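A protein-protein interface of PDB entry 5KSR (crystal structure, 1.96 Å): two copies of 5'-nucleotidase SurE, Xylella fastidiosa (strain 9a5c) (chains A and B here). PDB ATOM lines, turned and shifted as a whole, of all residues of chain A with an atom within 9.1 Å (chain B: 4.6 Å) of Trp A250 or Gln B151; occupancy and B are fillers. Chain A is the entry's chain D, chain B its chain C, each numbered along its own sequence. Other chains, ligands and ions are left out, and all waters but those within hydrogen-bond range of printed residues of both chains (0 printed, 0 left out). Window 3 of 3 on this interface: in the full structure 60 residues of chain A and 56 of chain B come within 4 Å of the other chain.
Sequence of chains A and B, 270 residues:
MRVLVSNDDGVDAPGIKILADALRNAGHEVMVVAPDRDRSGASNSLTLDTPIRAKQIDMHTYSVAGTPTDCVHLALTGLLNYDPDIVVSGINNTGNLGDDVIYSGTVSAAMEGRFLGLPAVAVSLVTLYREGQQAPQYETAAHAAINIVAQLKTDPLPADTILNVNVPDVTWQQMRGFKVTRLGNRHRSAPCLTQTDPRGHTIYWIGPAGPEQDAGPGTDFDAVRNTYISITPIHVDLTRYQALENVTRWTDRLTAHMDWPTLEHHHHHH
The backbone carbonyl oxygen (O) of Asp B155 lies within hydrogen-bond range of the indole nitrogen (NE1) of Trp A250, 3.0 Å away.
Hydrophobic or aromatic side chains of chain A within 4 Å of the printed part of chain B: Trp A250 and Met A258.
Along chain B the printed residues that touch a printed residue of chain A span positions 147 to 157.
Among the printed residues, 5 pairs touch across the chains.
Among the printed residues, no Asp or Glu carboxylate lies within 4 Å of a Lys or Arg side-chain nitrogen of the other chain.
Among the printed residues, merely in contact across the chains: Asn A246 with Leu B157, Trp A250 with Gln B151, Trp A250 with Leu B152 and Met A258 with Asn B147.
No position is printed for both chains.
Of the 5 pairs that touch across the chains among the printed residues, none has its exchanged pair printed and touching as well.
O of Gln B151 sits at hydrogen-bond distance from OG1 of Thr B154 (3.0 Å).
Printed residues of chain B within 4 Å of Asn A246: Leu B157.
Trp A250 touches just these residues of chain B: Gln B151, Leu B152 and Asp B155.
His A257 touches none of the printed residues of chain B.
Of the printed residues of chain B, Met A258 touches Asn B147 (3.9 Å).
Of the printed residues of chain A, Asn B147 touches Met A258.
Val B149 touches none of the printed residues of chain A.
No residue of chain A comes within 4 Å of Ala B150.
Gln B151 touches one residue of chain A.
Leu B152 touches just one residue of chain A: Trp A250 (3.7 Å).
Asp B155 touches just one residue of chain A: Trp A250 (3.0 Å).
Of the printed residues of chain A, Leu B157 touches Asn A246.
The nearest residue of chain B that does not touch Trp A250 is Leu B157 (4.2 Å).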
ATOM      1  N   ALA A 243      -9.192 -18.212  -3.245  1.00  0.00           N
ATOM      2  CA  ALA A 243     -10.450 -18.965  -3.044  1.00  0.00           C
ATOM      3  C   ALA A 243     -11.097 -18.908  -1.626  1.00  0.00           C
ATOM      4  O   ALA A 243     -12.178 -19.471  -1.415  1.00  0.00           O
ATOM      5  CB  ALA A 243     -10.276 -20.436  -3.492  1.00  0.00           C
ATOM      6  N   LEU A 244     -10.455 -18.242  -0.662  1.00  0.00           N
ATOM      7  CA  LEU A 244     -10.972 -18.233   0.721  1.00  0.00           C
ATOM      8  C   LEU A 244     -12.375 -17.614   0.897  1.00  0.00           C
ATOM      9  O   LEU A 244     -13.242 -18.201   1.555  1.00  0.00           O
ATOM     10  CB  LEU A 244      -9.963 -17.589   1.693  1.00  0.00           C
ATOM     11  CG  LEU A 244      -8.675 -18.357   2.009  1.00  0.00           C
ATOM     12  CD1 LEU A 244      -7.659 -17.488   2.773  1.00  0.00           C
ATOM     13  CD2 LEU A 244      -8.948 -19.689   2.760  1.00  0.00           C
ATOM     14  N   GLU A 245     -12.612 -16.441   0.310  1.00  0.00           N
ATOM     15  CA  GLU A 245     -13.896 -15.758   0.502  1.00  0.00           C
ATOM     16  C   GLU A 245     -15.074 -16.582  -0.023  1.00  0.00           C
ATOM     17  O   GLU A 245     -16.132 -16.632   0.591  1.00  0.00           O
ATOM     18  CB  GLU A 245     -13.884 -14.360  -0.126  1.00  0.00           C
ATOM     19  N   ASN A 246     -14.876 -17.258  -1.142  1.00  0.00           N
ATOM     20  CA  ASN A 246     -15.932 -18.087  -1.727  1.00  0.00           C
ATOM     21  C   ASN A 246     -16.240 -19.378  -0.941  1.00  0.00           C
ATOM     22  O   ASN A 246     -17.399 -19.796  -0.829  1.00  0.00           O
ATOM     23  CB  ASN A 246     -15.581 -18.423  -3.180  1.00  0.00           C
ATOM     24  CG  ASN A 246     -16.758 -18.973  -3.946  1.00  0.00           C
ATOM     25  OD1 ASN A 246     -17.701 -18.243  -4.261  1.00  0.00           O
ATOM     26  ND2 ASN A 246     -16.714 -20.263  -4.254  1.00  0.00           N
ATOM     27  N   VAL A 247     -15.200 -20.003  -0.402  1.00  0.00           N
ATOM     28  CA  VAL A 247     -15.342 -21.273   0.321  1.00  0.00           C
ATOM     29  C   VAL A 247     -16.034 -21.060   1.679  1.00  0.00           C
ATOM     30  O   VAL A 247     -16.745 -21.942   2.179  1.00  0.00           O
ATOM     31  CB  VAL A 247     -13.958 -21.993   0.437  1.00  0.00           C
ATOM     32  CG1 VAL A 247     -13.961 -23.181   1.428  1.00  0.00           C
ATOM     33  CG2 VAL A 247     -13.480 -22.464  -0.939  1.00  0.00           C
ATOM     34  N   THR A 248     -15.848 -19.872   2.252  1.00  0.00           N
ATOM     35  CA  THR A 248     -16.519 -19.488   3.500  1.00  0.00           C
ATOM     36  C   THR A 248     -18.051 -19.393   3.345  1.00  0.00           C
ATOM     37  O   THR A 248     -18.801 -19.853   4.216  1.00  0.00           O
ATOM     38  CB  THR A 248     -15.960 -18.144   4.055  1.00  0.00           C
ATOM     39  OG1 THR A 248     -14.547 -18.259   4.305  1.00  0.00           O
ATOM     40  CG2 THR A 248     -16.681 -17.728   5.341  1.00  0.00           C
ATOM     41  N   ARG A 249     -18.510 -18.794   2.246  1.00  0.00           N
ATOM     42  CA  ARG A 249     -19.946 -18.710   1.966  1.00  0.00           C
ATOM     43  C   ARG A 249     -20.540 -20.091   1.679  1.00  0.00           C
ATOM     44  O   ARG A 249     -21.690 -20.368   2.024  1.00  0.00           O
ATOM     45  CB  ARG A 249     -20.226 -17.772   0.786  1.00  0.00           C
ATOM     46  N   TRP A 250     -19.751 -20.945   1.036  1.00  0.00           N
ATOM     47  CA  TRP A 250     -20.127 -22.334   0.788  1.00  0.00           C
ATOM     48  C   TRP A 250     -20.339 -23.101   2.104  1.00  0.00           C
ATOM     49  O   TRP A 250     -21.341 -23.803   2.264  1.00  0.00           O
ATOM     50  CB  TRP A 250     -19.041 -23.009  -0.061  1.00  0.00           C
ATOM     51  CG  TRP A 250     -19.372 -24.396  -0.560  1.00  0.00           C
ATOM     52  CD1 TRP A 250     -19.935 -24.722  -1.761  1.00  0.00           C
ATOM     53  CD2 TRP A 250     -19.136 -25.639   0.120  1.00  0.00           C
ATOM     54  NE1 TRP A 250     -20.072 -26.091  -1.869  1.00  0.00           N
ATOM     55  CE2 TRP A 250     -19.595 -26.674  -0.724  1.00  0.00           C
ATOM     56  CE3 TRP A 250     -18.586 -25.976   1.363  1.00  0.00           C
ATOM     57  CZ2 TRP A 250     -19.518 -28.025  -0.366  1.00  0.00           C
ATOM     58  CZ3 TRP A 250     -18.516 -27.317   1.718  1.00  0.00           C
ATOM     59  CH2 TRP A 250     -18.976 -28.324   0.856  1.00  0.00           C
ATOM     60  N   THR A 251     -19.391 -22.957   3.037  1.00  0.00           N
ATOM     61  CA  THR A 251     -19.421 -23.660   4.326  1.00  0.00           C
ATOM     62  C   THR A 251     -20.573 -23.140   5.209  1.00  0.00           C
ATOM     63  O   THR A 251     -21.100 -23.872   6.053  1.00  0.00           O
ATOM     64  CB  THR A 251     -18.007 -23.620   5.041  1.00  0.00           C
ATOM     65  OG1 THR A 251     -17.015 -24.205   4.183  1.00  0.00           O
ATOM     66  CG2 THR A 251     -17.981 -24.410   6.348  1.00  0.00           C
ATOM     67  N   ASP A 252     -20.989 -21.891   4.989  1.00  0.00           N
ATOM     68  CA  ASP A 252     -22.154 -21.330   5.683  1.00  0.00           C
ATOM     69  C   ASP A 252     -23.464 -22.026   5.261  1.00  0.00           C
ATOM     70  O   ASP A 252     -24.285 -22.411   6.109  1.00  0.00           O
ATOM     71  CB  ASP A 252     -22.278 -19.816   5.437  1.00  0.00           C
ATOM     72  CG  ASP A 252     -21.222 -18.984   6.187  1.00  0.00           C
ATOM     73  OD1 ASP A 252     -20.533 -19.510   7.086  1.00  0.00           O
ATOM     74  OD2 ASP A 252     -21.107 -17.776   5.880  1.00  0.00           O
ATOM     75  N   ARG A 253     -23.672 -22.174   3.952  1.00  0.00           N
ATOM     76  CA  ARG A 253     -24.862 -22.878   3.453  1.00  0.00           C
ATOM     77  C   ARG A 253     -24.889 -24.359   3.868  1.00  0.00           C
ATOM     78  O   ARG A 253     -25.961 -24.954   3.987  1.00  0.00           O
ATOM     79  CB  ARG A 253     -24.993 -22.748   1.931  1.00  0.00           C
ATOM     80  CG  ARG A 253     -25.199 -21.323   1.431  1.00  0.00           C
ATOM     81  N   LEU A 254     -23.712 -24.945   4.089  1.00  0.00           N
ATOM     82  CA  LEU A 254     -23.623 -26.337   4.543  1.00  0.00           C
ATOM     83  C   LEU A 254     -24.201 -26.509   5.946  1.00  0.00           C
ATOM     84  O   LEU A 254     -25.057 -27.367   6.173  1.00  0.00           O
ATOM     85  CB  LEU A 254     -22.176 -26.847   4.505  1.00  0.00           C
ATOM     86  CG  LEU A 254     -21.844 -28.175   5.212  1.00  0.00           C
ATOM     87  CD1 LEU A 254     -22.653 -29.347   4.662  1.00  0.00           C
ATOM     88  CD2 LEU A 254     -20.346 -28.480   5.142  1.00  0.00           C
ATOM     89  N   THR A 255     -23.741 -25.684   6.880  1.00  0.00           N
ATOM     90  CA  THR A 255     -24.120 -25.837   8.279  1.00  0.00           C
ATOM     91  C   THR A 255     -25.568 -25.443   8.561  1.00  0.00           C
ATOM     92  O   THR A 255     -26.184 -25.963   9.491  1.00  0.00           O
ATOM     93  CB  THR A 255     -23.187 -25.045   9.203  1.00  0.00           C
ATOM     94  OG1 THR A 255     -23.196 -23.666   8.815  1.00  0.00           O
ATOM     95  CG2 THR A 255     -21.782 -25.580   9.105  1.00  0.00           C
ATOM     96  N   ALA A 256     -26.112 -24.527   7.766  1.00  0.00           N
ATOM     97  CA  ALA A 256     -27.505 -24.125   7.938  1.00  0.00           C
ATOM     98  C   ALA A 256     -28.432 -25.275   7.557  1.00  0.00           C
ATOM     99  O   ALA A 256     -29.532 -25.408   8.094  1.00  0.00           O
ATOM    100  CB  ALA A 256     -27.815 -22.884   7.108  1.00  0.00           C
ATOM    101  N   HIS A 257     -27.960 -26.107   6.633  1.00  0.00           N
ATOM    102  CA  HIS A 257     -28.715 -27.239   6.108  1.00  0.00           C
ATOM    103  C   HIS A 257     -28.882 -28.367   7.130  1.00  0.00           C
ATOM    104  O   HIS A 257     -30.001 -28.677   7.547  1.00  0.00           O
ATOM    105  CB  HIS A 257     -28.032 -27.766   4.841  1.00  0.00           C
ATOM    106  CG  HIS A 257     -28.666 -28.999   4.275  1.00  0.00           C
ATOM    107  ND1 HIS A 257     -29.956 -29.019   3.789  1.00  0.00           N
ATOM    108  CD2 HIS A 257     -28.181 -30.253   4.107  1.00  0.00           C
ATOM    109  CE1 HIS A 257     -30.240 -30.233   3.350  1.00  0.00           C
ATOM    110  NE2 HIS A 257     -29.180 -31.000   3.532  1.00  0.00           N
ATOM    111  N   MET A 258     -27.770 -28.977   7.530  1.00  0.00           N
ATOM    112  CA  MET A 258     -27.802 -30.097   8.467  1.00  0.00           C
ATOM    113  C   MET A 258     -28.319 -29.697   9.851  1.00  0.00           C
ATOM    114  O   MET A 258     -29.130 -30.409  10.453  1.00  0.00           O
ATOM    115  CB  MET A 258     -26.421 -30.746   8.571  1.00  0.00           C
ATOM    116  CG  MET A 258     -25.282 -29.767   8.788  1.00  0.00           C
ATOM    117  SD  MET A 258     -23.689 -30.446   8.289  1.00  0.00           S
ATOM    118  CE  MET A 258     -23.540 -31.857   9.384  1.00  0.00           C
ATOM    119  N   ASN B 147     -22.073 -35.682   4.260  1.00  0.00           N
ATOM    120  CA  ASN B 147     -22.708 -34.376   4.121  1.00  0.00           C
ATOM    121  C   ASN B 147     -21.974 -33.462   3.112  1.00  0.00           C
ATOM    122  O   ASN B 147     -22.617 -32.754   2.325  1.00  0.00           O
ATOM    123  CB  ASN B 147     -22.904 -33.711   5.492  1.00  0.00           C
ATOM    124  CG  ASN B 147     -24.187 -34.188   6.200  1.00  0.00           C
ATOM    125  OD1 ASN B 147     -25.297 -33.788   5.828  1.00  0.00           O
ATOM    126  ND2 ASN B 147     -24.033 -35.037   7.222  1.00  0.00           N
ATOM    127  N   ILE B 148     -20.639 -33.503   3.119  1.00  0.00           N
ATOM    128  CA  ILE B 148     -19.845 -32.724   2.176  1.00  0.00           C
ATOM    129  C   ILE B 148     -20.118 -33.188   0.723  1.00  0.00           C
ATOM    130  O   ILE B 148     -20.270 -32.361  -0.183  1.00  0.00           O
ATOM    131  CB  ILE B 148     -18.307 -32.746   2.554  1.00  0.00           C
ATOM    132  CG1 ILE B 148     -18.056 -31.907   3.815  1.00  0.00           C
ATOM    133  CG2 ILE B 148     -17.428 -32.249   1.388  1.00  0.00           C
ATOM    134  CD1 ILE B 148     -16.637 -32.041   4.409  1.00  0.00           C
ATOM    135  N   VAL B 149     -20.220 -34.497   0.503  1.00  0.00           N
ATOM    136  CA  VAL B 149     -20.526 -35.020  -0.830  1.00  0.00           C
ATOM    137  C   VAL B 149     -21.898 -34.567  -1.388  1.00  0.00           C
ATOM    138  O   VAL B 149     -21.976 -34.074  -2.522  1.00  0.00           O
ATOM    139  CB  VAL B 149     -20.377 -36.568  -0.903  1.00  0.00           C
ATOM    140  CG1 VAL B 149     -20.950 -37.108  -2.197  1.00  0.00           C
ATOM    141  CG2 VAL B 149     -18.903 -36.973  -0.763  1.00  0.00           C
ATOM    142  N   ALA B 150     -22.966 -34.713  -0.603  1.00  0.00           N
ATOM    143  CA  ALA B 150     -24.294 -34.330  -1.093  1.00  0.00           C
ATOM    144  C   ALA B 150     -24.387 -32.832  -1.391  1.00  0.00           C
ATOM    145  O   ALA B 150     -25.122 -32.413  -2.293  1.00  0.00           O
ATOM    146  CB  ALA B 150     -25.384 -34.750  -0.119  1.00  0.00           C
ATOM    147  N   GLN B 151     -23.629 -32.035  -0.643  1.00  0.00           N
ATOM    148  CA  GLN B 151     -23.623 -30.590  -0.834  1.00  0.00           C
ATOM    149  C   GLN B 151     -22.887 -30.127  -2.104  1.00  0.00           C
ATOM    150  O   GLN B 151     -23.284 -29.138  -2.721  1.00  0.00           O
ATOM    151  CB  GLN B 151     -23.061 -29.887   0.397  1.00  0.00           C
ATOM    152  CG  GLN B 151     -23.301 -28.382   0.424  1.00  0.00           C
ATOM    153  CD  GLN B 151     -24.733 -28.009   0.793  1.00  0.00           C
ATOM    154  OE1 GLN B 151     -25.421 -28.737   1.518  1.00  0.00           O
ATOM    155  NE2 GLN B 151     -25.187 -26.863   0.292  1.00  0.00           N
ATOM    156  N   LEU B 152     -21.825 -30.831  -2.496  1.00  0.00           N
ATOM    157  CA  LEU B 152     -21.095 -30.485  -3.717  1.00  0.00           C
ATOM    158  C   LEU B 152     -21.910 -30.841  -4.969  1.00  0.00           C
ATOM    159  O   LEU B 152     -21.635 -30.345  -6.065  1.00  0.00           O
ATOM    160  CB  LEU B 152     -19.714 -31.168  -3.758  1.00  0.00           C
ATOM    161  CG  LEU B 152     -18.539 -30.631  -2.922  1.00  0.00           C
ATOM    162  CD1 LEU B 152     -17.410 -31.655  -2.854  1.00  0.00           C
ATOM    163  CD2 LEU B 152     -17.997 -29.293  -3.455  1.00  0.00           C
ATOM    164  N   LYS B 153     -22.920 -31.692  -4.791  1.00  0.00           N
ATOM    165  CA  LYS B 153     -23.754 -32.158  -5.901  1.00  0.00           C
ATOM    166  C   LYS B 153     -24.716 -31.076  -6.380  1.00  0.00           C
ATOM    167  O   LYS B 153     -25.105 -31.046  -7.549  1.00  0.00           O
ATOM    168  CB  LYS B 153     -24.531 -33.412  -5.490  1.00  0.00           C
ATOM    169  N   THR B 154     -25.098 -30.194  -5.467  1.00  0.00           N
ATOM    170  CA  THR B 154     -25.986 -29.086  -5.790  1.00  0.00           C
ATOM    171  C   THR B 154     -25.186 -27.822  -6.106  1.00  0.00           C
ATOM    172  O   THR B 154     -25.487 -27.097  -7.055  1.00  0.00           O
ATOM    173  CB  THR B 154     -26.927 -28.789  -4.616  1.00  0.00           C
ATOM    174  OG1 THR B 154     -26.146 -28.477  -3.456  1.00  0.00           O
ATOM    175  CG2 THR B 154     -27.790 -30.000  -4.316  1.00  0.00           C
ATOM    176  N   ASP B 155     -24.154 -27.579  -5.304  1.00  0.00           N
ATOM    177  CA  ASP B 155     -23.382 -26.348  -5.362  1.00  0.00           C
ATOM    178  C   ASP B 155     -21.906 -26.690  -5.568  1.00  0.00           C
ATOM    179  O   ASP B 155     -21.142 -26.747  -4.608  1.00  0.00           O
ATOM    180  CB  ASP B 155     -23.583 -25.577  -4.050  1.00  0.00           C
ATOM    181  CG  ASP B 155     -22.962 -24.189  -4.067  1.00  0.00           C
ATOM    182  OD1 ASP B 155     -22.170 -23.880  -4.980  1.00  0.00           O
ATOM    183  OD2 ASP B 155     -23.261 -23.400  -3.142  1.00  0.00           O
ATOM    184  N   LEU B 157     -17.835 -26.514  -7.056  1.00  0.00           N
ATOM    185  CA  LEU B 157     -16.782 -25.526  -6.887  1.00  0.00           C
ATOM    186  C   LEU B 157     -16.054 -25.329  -8.203  1.00  0.00           C
ATOM    187  O   LEU B 157     -15.732 -26.296  -8.891  1.00  0.00           O
ATOM    188  CB  LEU B 157     -15.814 -25.953  -5.786  1.00  0.00           C
ATOM    189  CG  LEU B 157     -16.359 -25.735  -4.376  1.00  0.00           C
ATOM    190  CD1 LEU B 157     -15.483 -26.414  -3.328  1.00  0.00           C
ATOM    191  CD2 LEU B 157     -16.483 -24.245  -4.096  1.00  0.00           C
